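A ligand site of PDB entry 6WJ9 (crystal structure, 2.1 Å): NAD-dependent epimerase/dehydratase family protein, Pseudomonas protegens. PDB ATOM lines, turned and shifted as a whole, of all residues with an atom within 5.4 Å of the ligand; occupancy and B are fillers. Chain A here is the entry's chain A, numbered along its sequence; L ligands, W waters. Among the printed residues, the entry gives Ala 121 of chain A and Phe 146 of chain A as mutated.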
ATOM      1  N   GLY A  10      33.167 -25.380  17.473  1.00  0.00           N
ATOM      2  CA  GLY A  10      31.786 -25.166  17.858  1.00  0.00           C
ATOM      3  C   GLY A  10      31.004 -24.300  16.890  1.00  0.00           C
ATOM      4  O   GLY A  10      29.997 -23.707  17.282  1.00  0.00           O
ATOM      5  N   GLY A  11      31.450 -24.202  15.638  1.00  0.00           N
ATOM      6  CA  GLY A  11      30.826 -23.323  14.665  1.00  0.00           C
ATOM      7  C   GLY A  11      29.448 -23.755  14.207  1.00  0.00           C
ATOM      8  O   GLY A  11      28.764 -22.963  13.548  1.00  0.00           O
ATOM      9  N   ALA A  12      29.032 -24.988  14.510  1.00  0.00           N
ATOM     10  CA  ALA A  12      27.700 -25.461  14.162  1.00  0.00           C
ATOM     11  C   ALA A  12      26.647 -25.163  15.224  1.00  0.00           C
ATOM     12  O   ALA A  12      25.482 -25.498  15.025  1.00  0.00           O
ATOM     13  CB  ALA A  12      27.708 -26.970  13.879  1.00  0.00           C
ATOM     14  N   GLY A  13      27.032 -24.548  16.335  1.00  0.00           N
ATOM     15  CA  GLY A  13      26.123 -24.290  17.424  1.00  0.00           C
ATOM     16  C   GLY A  13      25.388 -22.967  17.280  1.00  0.00           C
ATOM     17  O   GLY A  13      25.358 -22.344  16.225  1.00  0.00           O
ATOM     18  N   PHE A  14      24.791 -22.549  18.407  1.00  0.00           N
ATOM     19  CA  PHE A  14      23.991 -21.329  18.453  1.00  0.00           C
ATOM     20  C   PHE A  14      24.840 -20.090  18.128  1.00  0.00           C
ATOM     21  O   PHE A  14      24.603 -19.412  17.127  1.00  0.00           O
ATOM     22  CB  PHE A  14      23.344 -21.236  19.853  1.00  0.00           C
ATOM     23  CG  PHE A  14      22.939 -19.847  20.293  1.00  0.00           C
ATOM     24  CD1 PHE A  14      22.240 -18.998  19.438  1.00  0.00           C
ATOM     25  CD2 PHE A  14      23.208 -19.422  21.588  1.00  0.00           C
ATOM     26  CE1 PHE A  14      21.869 -17.737  19.849  1.00  0.00           C
ATOM     27  CE2 PHE A  14      22.819 -18.151  22.010  1.00  0.00           C
ATOM     28  CZ  PHE A  14      22.157 -17.316  21.144  1.00  0.00           C
ATOM     29  N   ILE A  15      25.823 -19.802  18.971  1.00  0.00           N
ATOM     30  CA  ILE A  15      26.665 -18.621  18.742  1.00  0.00           C
ATOM     31  C   ILE A  15      27.553 -18.823  17.520  1.00  0.00           C
ATOM     32  O   ILE A  15      27.740 -17.911  16.705  1.00  0.00           O
ATOM     33  CB  ILE A  15      27.492 -18.322  20.006  1.00  0.00           C
ATOM     34  CG1 ILE A  15      26.576 -17.939  21.171  1.00  0.00           C
ATOM     35  CG2 ILE A  15      28.530 -17.235  19.718  1.00  0.00           C
ATOM     36  CD1 ILE A  15      27.290 -17.845  22.517  1.00  0.00           C
ATOM     37  N   GLY A  16      28.105 -20.036  17.366  1.00  0.00           N
ATOM     38  CA  GLY A  16      29.076 -20.281  16.323  1.00  0.00           C
ATOM     39  C   GLY A  16      28.510 -20.105  14.934  1.00  0.00           C
ATOM     40  O   GLY A  16      29.171 -19.558  14.045  1.00  0.00           O
ATOM     41  N   LEU A  33      34.908 -26.679  13.020  1.00  0.00           N
ATOM     42  CA  LEU A  33      35.180 -27.961  13.671  1.00  0.00           C
ATOM     43  C   LEU A  33      34.115 -28.163  14.733  1.00  0.00           C
ATOM     44  O   LEU A  33      34.034 -27.381  15.689  1.00  0.00           O
ATOM     45  CB  LEU A  33      36.575 -27.997  14.284  1.00  0.00           C
ATOM     46  CG  LEU A  33      36.907 -29.321  14.981  1.00  0.00           C
ATOM     47  CD1 LEU A  33      36.834 -30.435  13.950  1.00  0.00           C
ATOM     48  CD2 LEU A  33      38.282 -29.304  15.611  1.00  0.00           C
ATOM     49  N   ASP A  34      33.298 -29.206  14.565  1.00  0.00           N
ATOM     50  CA  ASP A  34      32.158 -29.423  15.451  1.00  0.00           C
ATOM     51  C   ASP A  34      31.860 -30.919  15.526  1.00  0.00           C
ATOM     52  O   ASP A  34      31.913 -31.618  14.511  1.00  0.00           O
ATOM     53  CB  ASP A  34      30.936 -28.655  14.943  1.00  0.00           C
ATOM     54  CG  ASP A  34      29.957 -28.342  16.042  1.00  0.00           C
ATOM     55  OD1 ASP A  34      29.272 -29.272  16.523  1.00  0.00           O
ATOM     56  OD2 ASP A  34      29.895 -27.168  16.455  1.00  0.00           O
ATOM     57  N   ASP A  35      31.554 -31.408  16.722  1.00  0.00           N
ATOM     58  CA  ASP A  35      31.200 -32.822  16.840  1.00  0.00           C
ATOM     59  C   ASP A  35      29.714 -33.070  16.669  1.00  0.00           C
ATOM     60  O   ASP A  35      29.277 -34.227  16.760  1.00  0.00           O
ATOM     61  CB  ASP A  35      31.666 -33.399  18.189  1.00  0.00           C
ATOM     62  CG  ASP A  35      30.907 -32.819  19.382  1.00  0.00           C
ATOM     63  OD1 ASP A  35      30.180 -31.822  19.230  1.00  0.00           O
ATOM     64  OD2 ASP A  35      31.073 -33.379  20.481  1.00  0.00           O
ATOM     65  N   LEU A  36      28.924 -32.012  16.422  1.00  0.00           N
ATOM     66  CA  LEU A  36      27.476 -32.096  16.230  1.00  0.00           C
ATOM     67  C   LEU A  36      26.777 -32.779  17.408  1.00  0.00           C
ATOM     68  O   LEU A  36      25.747 -33.452  17.246  1.00  0.00           O
ATOM     69  CB  LEU A  36      27.138 -32.789  14.905  1.00  0.00           C
ATOM     70  CG  LEU A  36      27.739 -32.151  13.643  1.00  0.00           C
ATOM     71  CD1 LEU A  36      27.303 -32.893  12.383  1.00  0.00           C
ATOM     72  CD2 LEU A  36      27.409 -30.666  13.540  1.00  0.00           C
ATOM     73  N   SER A  37      27.351 -32.617  18.598  1.00  0.00           N
ATOM     74  CA  SER A  37      26.673 -33.061  19.822  1.00  0.00           C
ATOM     75  C   SER A  37      25.422 -32.221  20.075  1.00  0.00           C
ATOM     76  O   SER A  37      24.324 -32.753  20.232  1.00  0.00           O
ATOM     77  CB  SER A  37      27.645 -32.999  21.000  1.00  0.00           C
ATOM     78  OG  SER A  37      28.282 -31.738  21.071  1.00  0.00           O
ATOM     79  N   THR A  38      25.581 -30.896  20.122  1.00  0.00           N
ATOM     80  CA  THR A  38      24.435 -29.991  20.092  1.00  0.00           C
ATOM     81  C   THR A  38      24.378 -29.131  18.838  1.00  0.00           C
ATOM     82  O   THR A  38      23.304 -28.616  18.507  1.00  0.00           O
ATOM     83  CB  THR A  38      24.412 -29.064  21.321  1.00  0.00           C
ATOM     84  OG1 THR A  38      25.588 -28.242  21.333  1.00  0.00           O
ATOM     85  CG2 THR A  38      24.332 -29.882  22.625  1.00  0.00           C
ATOM     86  N   GLY A  39      25.499 -28.951  18.140  1.00  0.00           N
ATOM     87  CA  GLY A  39      25.461 -28.230  16.893  1.00  0.00           C
ATOM     88  C   GLY A  39      24.691 -28.988  15.825  1.00  0.00           C
ATOM     89  O   GLY A  39      24.541 -30.203  15.883  1.00  0.00           O
ATOM     90  N   LYS A  40      24.191 -28.241  14.844  1.00  0.00           N
ATOM     91  CA  LYS A  40      23.344 -28.801  13.783  1.00  0.00           C
ATOM     92  C   LYS A  40      23.796 -28.252  12.437  1.00  0.00           C
ATOM     93  O   LYS A  40      24.038 -27.058  12.299  1.00  0.00           O
ATOM     94  CB  LYS A  40      21.861 -28.448  13.979  1.00  0.00           C
ATOM     95  CG  LYS A  40      21.236 -28.964  15.249  1.00  0.00           C
ATOM     96  CD  LYS A  40      19.810 -28.475  15.372  1.00  0.00           C
ATOM     97  N   GLY A  56      34.107 -33.734  14.170  1.00  0.00           N
ATOM     98  CA  GLY A  56      34.938 -34.489  15.078  1.00  0.00           C
ATOM     99  C   GLY A  56      35.111 -33.760  16.403  1.00  0.00           C
ATOM    100  O   GLY A  56      34.532 -32.690  16.630  1.00  0.00           O
ATOM    101  N   ASP A  57      35.938 -34.369  17.245  1.00  0.00           N
ATOM    102  CA  ASP A  57      36.131 -33.940  18.627  1.00  0.00           C
ATOM    103  C   ASP A  57      37.258 -32.911  18.695  1.00  0.00           C
ATOM    104  O   ASP A  57      38.403 -33.209  18.343  1.00  0.00           O
ATOM    105  CB  ASP A  57      36.458 -35.152  19.492  1.00  0.00           C
ATOM    106  CG  ASP A  57      36.609 -34.832  20.979  1.00  0.00           C
ATOM    107  OD1 ASP A  57      36.509 -33.643  21.402  1.00  0.00           O
ATOM    108  OD2 ASP A  57      36.837 -35.793  21.728  1.00  0.00           O
ATOM    109  N   ALA A  58      36.940 -31.714  19.186  1.00  0.00           N
ATOM    110  CA  ALA A  58      37.945 -30.669  19.307  1.00  0.00           C
ATOM    111  C   ALA A  58      39.052 -31.016  20.282  1.00  0.00           C
ATOM    112  O   ALA A  58      40.116 -30.374  20.256  1.00  0.00           O
ATOM    113  CB  ALA A  58      37.260 -29.348  19.705  1.00  0.00           C
ATOM    114  N   ALA A  59      38.853 -32.011  21.151  1.00  0.00           N
ATOM    115  CA  ALA A  59      39.944 -32.507  21.985  1.00  0.00           C
ATOM    116  C   ALA A  59      40.864 -33.474  21.254  1.00  0.00           C
ATOM    117  O   ALA A  59      41.840 -33.943  21.856  1.00  0.00           O
ATOM    118  CB  ALA A  59      39.374 -33.190  23.235  1.00  0.00           C
ATOM    119  N   HIS A  76      37.328 -20.029  19.446  1.00  0.00           N
ATOM    120  CA  HIS A  76      37.227 -21.315  20.139  1.00  0.00           C
ATOM    121  C   HIS A  76      35.948 -21.302  20.959  1.00  0.00           C
ATOM    122  O   HIS A  76      35.925 -20.846  22.106  1.00  0.00           O
ATOM    123  CB  HIS A  76      38.462 -21.585  20.989  1.00  0.00           C
ATOM    124  CG  HIS A  76      38.389 -22.858  21.776  1.00  0.00           C
ATOM    125  ND1 HIS A  76      37.912 -24.038  21.242  1.00  0.00           N
ATOM    126  CD2 HIS A  76      38.753 -23.136  23.056  1.00  0.00           C
ATOM    127  CE1 HIS A  76      37.977 -24.994  22.151  1.00  0.00           C
ATOM    128  NE2 HIS A  76      38.474 -24.471  23.267  1.00  0.00           N
ATOM    129  N   LEU A  77      34.870 -21.806  20.358  1.00  0.00           N
ATOM    130  CA  LEU A  77      33.557 -21.861  20.978  1.00  0.00           C
ATOM    131  C   LEU A  77      33.166 -23.265  21.426  1.00  0.00           C
ATOM    132  O   LEU A  77      32.206 -23.397  22.196  1.00  0.00           O
ATOM    133  CB  LEU A  77      32.486 -21.315  20.004  1.00  0.00           C
ATOM    134  CG  LEU A  77      32.742 -19.907  19.420  1.00  0.00           C
ATOM    135  CD1 LEU A  77      31.699 -19.481  18.375  1.00  0.00           C
ATOM    136  CD2 LEU A  77      32.816 -18.858  20.535  1.00  0.00           C
ATOM    137  N   ALA A  78      33.878 -24.301  20.984  1.00  0.00           N
ATOM    138  CA  ALA A  78      33.473 -25.658  21.318  1.00  0.00           C
ATOM    139  C   ALA A  78      33.596 -25.903  22.813  1.00  0.00           C
ATOM    140  O   ALA A  78      34.626 -25.603  23.430  1.00  0.00           O
ATOM    141  CB  ALA A  78      34.311 -26.679  20.545  1.00  0.00           C
ATOM    142  N   ALA A  79      32.527 -26.421  23.397  1.00  0.00           N
ATOM    143  CA  ALA A  79      32.462 -26.882  24.787  1.00  0.00           C
ATOM    144  C   ALA A  79      31.085 -27.510  24.946  1.00  0.00           C
ATOM    145  O   ALA A  79      30.190 -27.276  24.121  1.00  0.00           O
ATOM    146  CB  ALA A  79      32.657 -25.739  25.793  1.00  0.00           C
ATOM    147  N   VAL A  80      30.920 -28.316  25.984  1.00  0.00           N
ATOM    148  CA  VAL A  80      29.585 -28.743  26.392  1.00  0.00           C
ATOM    149  C   VAL A  80      28.978 -27.569  27.156  1.00  0.00           C
ATOM    150  O   VAL A  80      29.431 -27.240  28.260  1.00  0.00           O
ATOM    151  CB  VAL A  80      29.612 -30.016  27.236  1.00  0.00           C
ATOM    152  CG1 VAL A  80      28.196 -30.364  27.736  1.00  0.00           C
ATOM    153  CG2 VAL A  80      30.193 -31.181  26.407  1.00  0.00           C
ATOM    154  N   ALA A  81      27.972 -26.911  26.563  1.00  0.00           N
ATOM    155  CA  ALA A  81      27.530 -25.622  27.081  1.00  0.00           C
ATOM    156  C   ALA A  81      26.720 -25.775  28.359  1.00  0.00           C
ATOM    157  O   ALA A  81      26.698 -24.858  29.189  1.00  0.00           O
ATOM    158  CB  ALA A  81      26.704 -24.884  26.018  1.00  0.00           C
ATOM    159  N   SER A  96      35.924 -31.907  26.787  1.00  0.00           N
ATOM    160  CA  SER A  96      35.392 -30.874  25.903  1.00  0.00           C
ATOM    161  C   SER A  96      35.635 -29.463  26.444  1.00  0.00           C
ATOM    162  O   SER A  96      35.896 -28.528  25.669  1.00  0.00           O
ATOM    163  CB  SER A  96      33.896 -31.088  25.679  1.00  0.00           C
ATOM    164  OG  SER A  96      33.663 -32.220  24.864  1.00  0.00           O
ATOM    165  N   ALA A 119      35.688 -18.206  24.241  1.00  0.00           N
ATOM    166  CA  ALA A 119      34.399 -18.094  24.924  1.00  0.00           C
ATOM    167  C   ALA A 119      34.542 -18.581  26.356  1.00  0.00           C
ATOM    168  O   ALA A 119      34.345 -19.760  26.655  1.00  0.00           O
ATOM    169  CB  ALA A 119      33.340 -18.908  24.182  1.00  0.00           C
ATOM    170  N   SER A 120      34.886 -17.660  27.260  1.00  0.00           N
ATOM    171  CA  SER A 120      34.778 -17.946  28.675  1.00  0.00           C
ATOM    172  C   SER A 120      33.364 -17.594  29.116  1.00  0.00           C
ATOM    173  O   SER A 120      32.469 -17.360  28.290  1.00  0.00           O
ATOM    174  CB  SER A 120      35.858 -17.205  29.480  1.00  0.00           C
ATOM    175  OG  SER A 120      35.983 -17.810  30.749  1.00  0.00           O
ATOM    176  N   ALA A 121      33.131 -17.510  30.431  1.00  0.00           N
ATOM    177  CA  ALA A 121      31.756 -17.501  30.947  1.00  0.00           C
ATOM    178  C   ALA A 121      31.677 -16.751  32.266  1.00  0.00           C
ATOM    179  O   ALA A 121      32.600 -16.815  33.092  1.00  0.00           O
ATOM    180  CB  ALA A 121      31.250 -18.938  31.121  1.00  0.00           C
ATOM    181  N   ALA A 122      30.546 -16.067  32.491  1.00  0.00           N
ATOM    182  CA  ALA A 122      30.294 -15.449  33.791  1.00  0.00           C
ATOM    183  C   ALA A 122      30.291 -16.462  34.939  1.00  0.00           C
ATOM    184  O   ALA A 122      30.497 -16.078  36.092  1.00  0.00           O
ATOM    185  CB  ALA A 122      28.972 -14.682  33.761  1.00  0.00           C
ATOM    186  N   PHE A 146      32.292 -27.334  34.655  1.00  0.00           N
ATOM    187  CA  PHE A 146      32.272 -26.417  33.513  1.00  0.00           C
ATOM    188  C   PHE A 146      32.940 -25.084  33.860  1.00  0.00           C
ATOM    189  O   PHE A 146      33.798 -24.582  33.122  1.00  0.00           O
ATOM    190  CB  PHE A 146      30.832 -26.190  33.026  1.00  0.00           C
ATOM    191  CG  PHE A 146      30.666 -25.008  32.097  1.00  0.00           C
ATOM    192  CD1 PHE A 146      30.793 -25.166  30.719  1.00  0.00           C
ATOM    193  CD2 PHE A 146      30.386 -23.732  32.590  1.00  0.00           C
ATOM    194  CE1 PHE A 146      30.639 -24.091  29.861  1.00  0.00           C
ATOM    195  CE2 PHE A 146      30.234 -22.648  31.736  1.00  0.00           C
ATOM    196  CZ  PHE A 146      30.367 -22.824  30.373  1.00  0.00           C
ATOM    197  N   LYS A 150      36.424 -23.563  32.327  1.00  0.00           N
ATOM    198  CA  LYS A 150      36.524 -22.283  31.621  1.00  0.00           C
ATOM    199  C   LYS A 150      37.631 -21.431  32.212  1.00  0.00           C
ATOM    200  O   LYS A 150      38.437 -20.843  31.476  1.00  0.00           O
ATOM    201  CB  LYS A 150      35.191 -21.540  31.688  1.00  0.00           C
ATOM    202  CG  LYS A 150      34.072 -22.122  30.775  1.00  0.00           C
ATOM    203  CD  LYS A 150      34.550 -22.198  29.336  1.00  0.00           C
ATOM    204  CE  LYS A 150      33.398 -22.451  28.353  1.00  0.00           C
ATOM    205  NZ  LYS A 150      33.887 -22.518  26.941  1.00  0.00           N
ATOM    206  N   PHE A 173      31.271 -14.454  28.595  1.00  0.00           N
ATOM    207  CA  PHE A 173      29.902 -14.217  28.154  1.00  0.00           C
ATOM    208  C   PHE A 173      28.969 -14.170  29.347  1.00  0.00           C
ATOM    209  O   PHE A 173      29.013 -15.051  30.216  1.00  0.00           O
ATOM    210  CB  PHE A 173      29.396 -15.317  27.206  1.00  0.00           C
ATOM    211  CG  PHE A 173      30.182 -15.487  25.927  1.00  0.00           C
ATOM    212  CD1 PHE A 173      31.156 -14.570  25.547  1.00  0.00           C
ATOM    213  CD2 PHE A 173      29.928 -16.578  25.103  1.00  0.00           C
ATOM    214  CE1 PHE A 173      31.882 -14.750  24.385  1.00  0.00           C
ATOM    215  CE2 PHE A 173      30.633 -16.760  23.926  1.00  0.00           C
ATOM    216  CZ  PHE A 173      31.616 -15.848  23.557  1.00  0.00           C
ATOM    217  N   PHE A 174      28.092 -13.156  29.372  1.00  0.00           N
ATOM    218  CA  PHE A 174      26.951 -13.191  30.270  1.00  0.00           C
ATOM    219  C   PHE A 174      25.805 -13.891  29.535  1.00  0.00           C
ATOM    220  O   PHE A 174      26.070 -14.879  28.843  1.00  0.00           O
ATOM    221  CB  PHE A 174      26.662 -11.771  30.792  1.00  0.00           C
ATOM    222  CG  PHE A 174      27.576 -11.387  31.959  1.00  0.00           C
ATOM    223  CD1 PHE A 174      28.955 -11.300  31.757  1.00  0.00           C
ATOM    224  CD2 PHE A 174      27.076 -11.224  33.244  1.00  0.00           C
ATOM    225  CE1 PHE A 174      29.817 -10.993  32.814  1.00  0.00           C
ATOM    226  CE2 PHE A 174      27.927 -10.919  34.310  1.00  0.00           C
ATOM    227  CZ  PHE A 174      29.312 -10.807  34.096  1.00  0.00           C
ATOM    228  N   ASN A 175      24.552 -13.451  29.665  1.00  0.00           N
ATOM    229  CA  ASN A 175      23.410 -14.279  29.228  1.00  0.00           C
ATOM    230  C   ASN A 175      23.068 -13.998  27.758  1.00  0.00           C
ATOM    231  O   ASN A 175      22.339 -13.049  27.449  1.00  0.00           O
ATOM    232  CB  ASN A 175      22.205 -14.063  30.132  1.00  0.00           C
ATOM    233  CG  ASN A 175      22.446 -14.617  31.543  1.00  0.00           C
ATOM    234  OD1 ASN A 175      23.183 -14.027  32.330  1.00  0.00           O
ATOM    235  ND2 ASN A 175      21.828 -15.746  31.854  1.00  0.00           N
ATOM    236  N   ILE A 176      23.596 -14.839  26.856  1.00  0.00           N
ATOM    237  CA  ILE A 176      23.394 -14.653  25.415  1.00  0.00           C
ATOM    238  C   ILE A 176      22.064 -15.267  25.007  1.00  0.00           C
ATOM    239  O   ILE A 176      21.652 -16.293  25.534  1.00  0.00           O
ATOM    240  CB  ILE A 176      24.558 -15.291  24.633  1.00  0.00           C
ATOM    241  CG1 ILE A 176      25.919 -14.934  25.265  1.00  0.00           C
ATOM    242  CG2 ILE A 176      24.464 -14.919  23.135  1.00  0.00           C
ATOM    243  CD1 ILE A 176      26.198 -13.453  25.439  1.00  0.00           C
ATOM    244  N   GLN A 181      19.118 -20.721  19.439  1.00  0.00           N
ATOM    245  CA  GLN A 181      19.418 -21.218  20.782  1.00  0.00           C
ATOM    246  C   GLN A 181      18.397 -22.296  21.151  1.00  0.00           C
ATOM    247  O   GLN A 181      17.190 -22.038  21.191  1.00  0.00           O
ATOM    248  CB  GLN A 181      19.413 -20.085  21.809  1.00  0.00           C
ATOM    249  CG  GLN A 181      19.891 -20.562  23.174  1.00  0.00           C
ATOM    250  CD  GLN A 181      19.977 -19.443  24.188  1.00  0.00           C
ATOM    251  OE1 GLN A 181      19.145 -18.543  24.200  1.00  0.00           O
ATOM    252  NE2 GLN A 181      20.996 -19.486  25.046  1.00  0.00           N
HETATM  253  P1  LIG L   1      26.062 -24.615  21.726  1.00  0.00           P
HETATM  254  O1  LIG L   1      25.916 -25.971  22.398  1.00  0.00           O
HETATM  255  O2  LIG L   1      24.993 -24.343  20.697  1.00  0.00           O
HETATM  256  O3  LIG L   1      27.479 -24.452  20.999  1.00  0.00           O
HETATM  257  C1  LIG L   1      28.412 -25.415  21.461  1.00  0.00           C
HETATM  258  C2  LIG L   1      28.961 -26.077  20.197  1.00  0.00           C
HETATM  259  O4  LIG L   1      30.161 -26.817  20.476  1.00  0.00           O
HETATM  260  C3  LIG L   1      27.961 -27.052  19.556  1.00  0.00           C
HETATM  261  O5  LIG L   1      27.967 -26.852  18.138  1.00  0.00           O
HETATM  262  C4  LIG L   1      28.559 -28.421  19.921  1.00  0.00           C
HETATM  263  O6  LIG L   1      28.207 -29.433  18.972  1.00  0.00           O
HETATM  264  C5  LIG L   1      30.068 -28.085  19.880  1.00  0.00           C
HETATM  265  N1  LIG L   1      30.889 -29.007  20.662  1.00  0.00           N
HETATM  266  C6  LIG L   1      30.666 -29.424  21.939  1.00  0.00           C
HETATM  267  N2  LIG L   1      31.592 -30.251  22.362  1.00  0.00           N
HETATM  268  C7  LIG L   1      32.463 -30.392  21.331  1.00  0.00           C
HETATM  269  C8  LIG L   1      33.640 -31.135  21.124  1.00  0.00           C
HETATM  270  N3  LIG L   1      34.178 -31.937  22.113  1.00  0.00           N
HETATM  271  N4  LIG L   1      34.248 -31.025  19.952  1.00  0.00           N
HETATM  272  C9  LIG L   1      33.740 -30.259  19.009  1.00  0.00           C
HETATM  273  N5  LIG L   1      32.643 -29.523  19.053  1.00  0.00           N
HETATM  274  C10 LIG L   1      32.034 -29.630  20.247  1.00  0.00           C
HETATM  275  O7  LIG L   1      25.985 -23.429  22.794  1.00  0.00           O
HETATM  276  P2  LIG L   1      26.476 -21.921  22.644  1.00  0.00           P
HETATM  277  O8  LIG L   1      25.489 -21.117  23.521  1.00  0.00           O
HETATM  278  O9  LIG L   1      26.557 -21.454  21.172  1.00  0.00           O
HETATM  279  O10 LIG L   1      27.928 -21.954  23.331  1.00  0.00           O
HETATM  280  C11 LIG L   1      29.005 -21.398  22.589  1.00  0.00           C
HETATM  281  C12 LIG L   1      30.179 -21.143  23.554  1.00  0.00           C
HETATM  282  O11 LIG L   1      29.859 -20.036  24.421  1.00  0.00           O
HETATM  283  C13 LIG L   1      30.378 -22.353  24.510  1.00  0.00           C
HETATM  284  O12 LIG L   1      31.775 -22.514  24.768  1.00  0.00           O
HETATM  285  C14 LIG L   1      29.650 -21.888  25.785  1.00  0.00           C
HETATM  286  O13 LIG L   1      30.129 -22.541  26.958  1.00  0.00           O
HETATM  287  C15 LIG L   1      29.994 -20.395  25.779  1.00  0.00           C
HETATM  288  N6  LIG L   1      29.012 -19.637  26.577  1.00  0.00           N
HETATM  289  C16 LIG L   1      27.754 -19.446  26.167  1.00  0.00           C
HETATM  290  C17 LIG L   1      26.841 -18.706  26.946  1.00  0.00           C
HETATM  291  C18 LIG L   1      25.424 -18.438  26.563  1.00  0.00           C
HETATM  292  O14 LIG L   1      24.758 -17.679  27.245  1.00  0.00           O
HETATM  293  N7  LIG L   1      24.936 -19.049  25.471  1.00  0.00           N
HETATM  294  C19 LIG L   1      27.292 -18.174  28.176  1.00  0.00           C
HETATM  295  C20 LIG L   1      28.614 -18.408  28.548  1.00  0.00           C
HETATM  296  C21 LIG L   1      29.451 -19.134  27.720  1.00  0.00           C
HETATM  297  O   HOH W   1      27.623 -22.315  28.506  1.00  0.00           O
HETATM  298  O   HOH W   2      24.576 -17.426  30.097  1.00  0.00           O
HETATM  299  O   HOH W   3      23.070 -25.679  19.313  1.00  0.00           O
HETATM  300  O   HOH W   4      23.206 -21.814  24.652  1.00  0.00           O
HETATM  301  O   HOH W   5      30.716 -32.997  23.150  1.00  0.00           O
HETATM  302  O   HOH W   6      21.778 -17.935  27.782  1.00  0.00           O
HETATM  303  O   HOH W   7      34.853 -22.647  23.998  1.00  0.00           O
HETATM  304  O   HOH W   8      26.787 -27.934  24.175  1.00  0.00           O
HETATM  305  O   HOH W   9      35.944 -34.116  24.078  1.00  0.00           O
HETATM  306  O   HOH W  10      23.242 -25.964  23.672  1.00  0.00           O
HETATM  307  O   HOH W  11      28.303 -22.296  19.113  1.00  0.00           O
HETATM  308  O   HOH W  12      27.764 -30.431  23.470  1.00  0.00           O
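The backbone NH (N) of Thr 38 sits at hydrogen-bond distance from an oxygen (O6) of the ligand, at 3.2 Å.
The side-chain hydroxyl (OG1) of Thr 38 sits at hydrogen-bond distance from an oxygen (O1) of the ligand (2.5 Å).
OD2 of Asp 34 is in hydrogen-bond range of O5 of the ligand, 2.6 Å away.
O12 of the ligand is in hydrogen-bond range of O of Leu 77, at 2.8 Å.
N3 of the ligand sits at hydrogen-bond distance from OG of Ser 96 (2.8 Å).
N of Ile 15 sits at hydrogen-bond distance from O9 of the ligand (2.8 Å).
O6 of the ligand sits at hydrogen-bond distance from N of Gly 39 (2.9 Å).
The backbone NH (N) of Ala 58 sits at hydrogen-bond distance from a nitrogen (N4) of the ligand (2.9 Å).
The backbone NH of Phe 14 is in hydrogen-bond range of an oxygen (O2) of the ligand, 2.9 Å away.
The side-chain carboxylate (OD1) of Asp 57 lies within hydrogen-bond range of a nitrogen (N3) of the ligand, at 3.0 Å.
An oxygen (O12) of the ligand sits at hydrogen-bond distance from the side-chain amino group (NZ) of Lys 150.
N of Asp 35 lies within hydrogen-bond range of N5 of the ligand, at 3.2 Å.
OD1 of Asp 35 lies close to O6 of the ligand (3.1 Å).
N of Gly 13 lies within hydrogen-bond range of O5 of the ligand (3.1 Å).
O14 of the ligand sits at hydrogen-bond distance from N of Ile 176, 3.1 Å away.
The backbone NH (N) of Ser 37 lies within hydrogen-bond range of an oxygen (O6) of the ligand (3.3 Å).
The side-chain hydroxyl (OG) of Ser 37 is in hydrogen-bond range of an oxygen (O6) of the ligand.
N of Leu 36 sits at hydrogen-bond distance from OD1 of Asp 34.
The side-chain carboxylate (OD2) of Asp 34 sits at hydrogen-bond distance from the backbone NH (N) of Gly 11 (3.4 Å).
The side-chain carboxylate (OD1) of Asp 57 sits at hydrogen-bond distance from the backbone NH (N) of Ala 59 (2.9 Å).
The backbone NH of Asp 35 is in hydrogen-bond range of the backbone carbonyl oxygen of Gly 56, at 3.2 Å.
The backbone carbonyl oxygen (O) of Ser 120 sits at hydrogen-bond distance from the backbone NH (N) of Phe 173.
The backbone carbonyl oxygen (O) of Phe 173 sits at hydrogen-bond distance from the backbone NH (N) of Ala 122, 2.9 Å away.
N of Gly 10 sits at hydrogen-bond distance from O of Leu 33, at 2.8 Å.
The backbone NH (N) of Lys 40 sits at hydrogen-bond distance from the backbone carbonyl oxygen (O) of Ala 12 (3.0 Å).
O of Phe 174 lies close to O14 of the ligand, at 3.5 Å.
Residues that only touch the ligand: Ala 79 (3.1 Å), Phe 146 (3.3 Å), Phe 173 (3.4 Å), Gly 56 (3.5 Å), Gly 10 (3.5 Å), Ser 120 (3.5 Å), Ala 78 (3.6 Å), Ala 81 (3.6 Å), Ala 12 (3.6 Å), Ala 119 (3.7 Å), Leu 36 (3.7 Å), Ala 121 (3.7 Å) and Gln 181 (3.99 Å).
Hydrophobic or aromatic side chains that line the ligand: Phe 14, Ile 15, Ala 58, Ala 78, Ala 79, Ala 81, Ala 119, Ala 121, Phe 146, Phe 173 and Ile 176.
Within 4 Å of the ligand: Gly 10, Ala 12, Gly 13, Phe 14, Ile 15, Asp 34, Asp 35, Leu 36, Ser 37, Thr 38, Gly 39, Gly 56, Asp 57, Ala 58, Leu 77, Ala 78, Ala 79, Ala 81, Ser 96, Ala 119, Ser 120, Ala 121, Phe 146, Lys 150, Phe 173, Phe 174, Ile 176 and Gln 181.
The nearest printed residue that does not touch the ligand is Asn 175 (4.1 Å).
Water W4 bridges O8 of the ligand (2.6 Å) and NE2 of Gln 181 (3.2 Å).
Water W8 lies within hydrogen-bond range of O1 of the ligand (2.8 Å), N of Ala 81 (2.9 Å), OG1 of Thr 38 (3.1 Å) and O of Ala 79 (3.5 Å).
Water W11 lies within hydrogen-bond range of O9 of the ligand, N of Gly 16 and O of Gly 10.
Water W2 lies within hydrogen-bond range of O14 of the ligand (2.9 Å) and O of Phe 174 (3.2 Å).
Water W5 lies within hydrogen-bond range of OD2 of Asp 35 (2.7 Å), N2 of the ligand (3.0 Å), OG of Ser 37 (3.4 Å) and OG of Ser 96 (3.5 Å).
Water W9 lies within hydrogen-bond range of the side-chain carboxylate of Asp 57 (2.8 Å), the side-chain hydroxyl of Ser 96 (3.1 Å) and a nitrogen (N3) of the ligand (3.4 Å).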
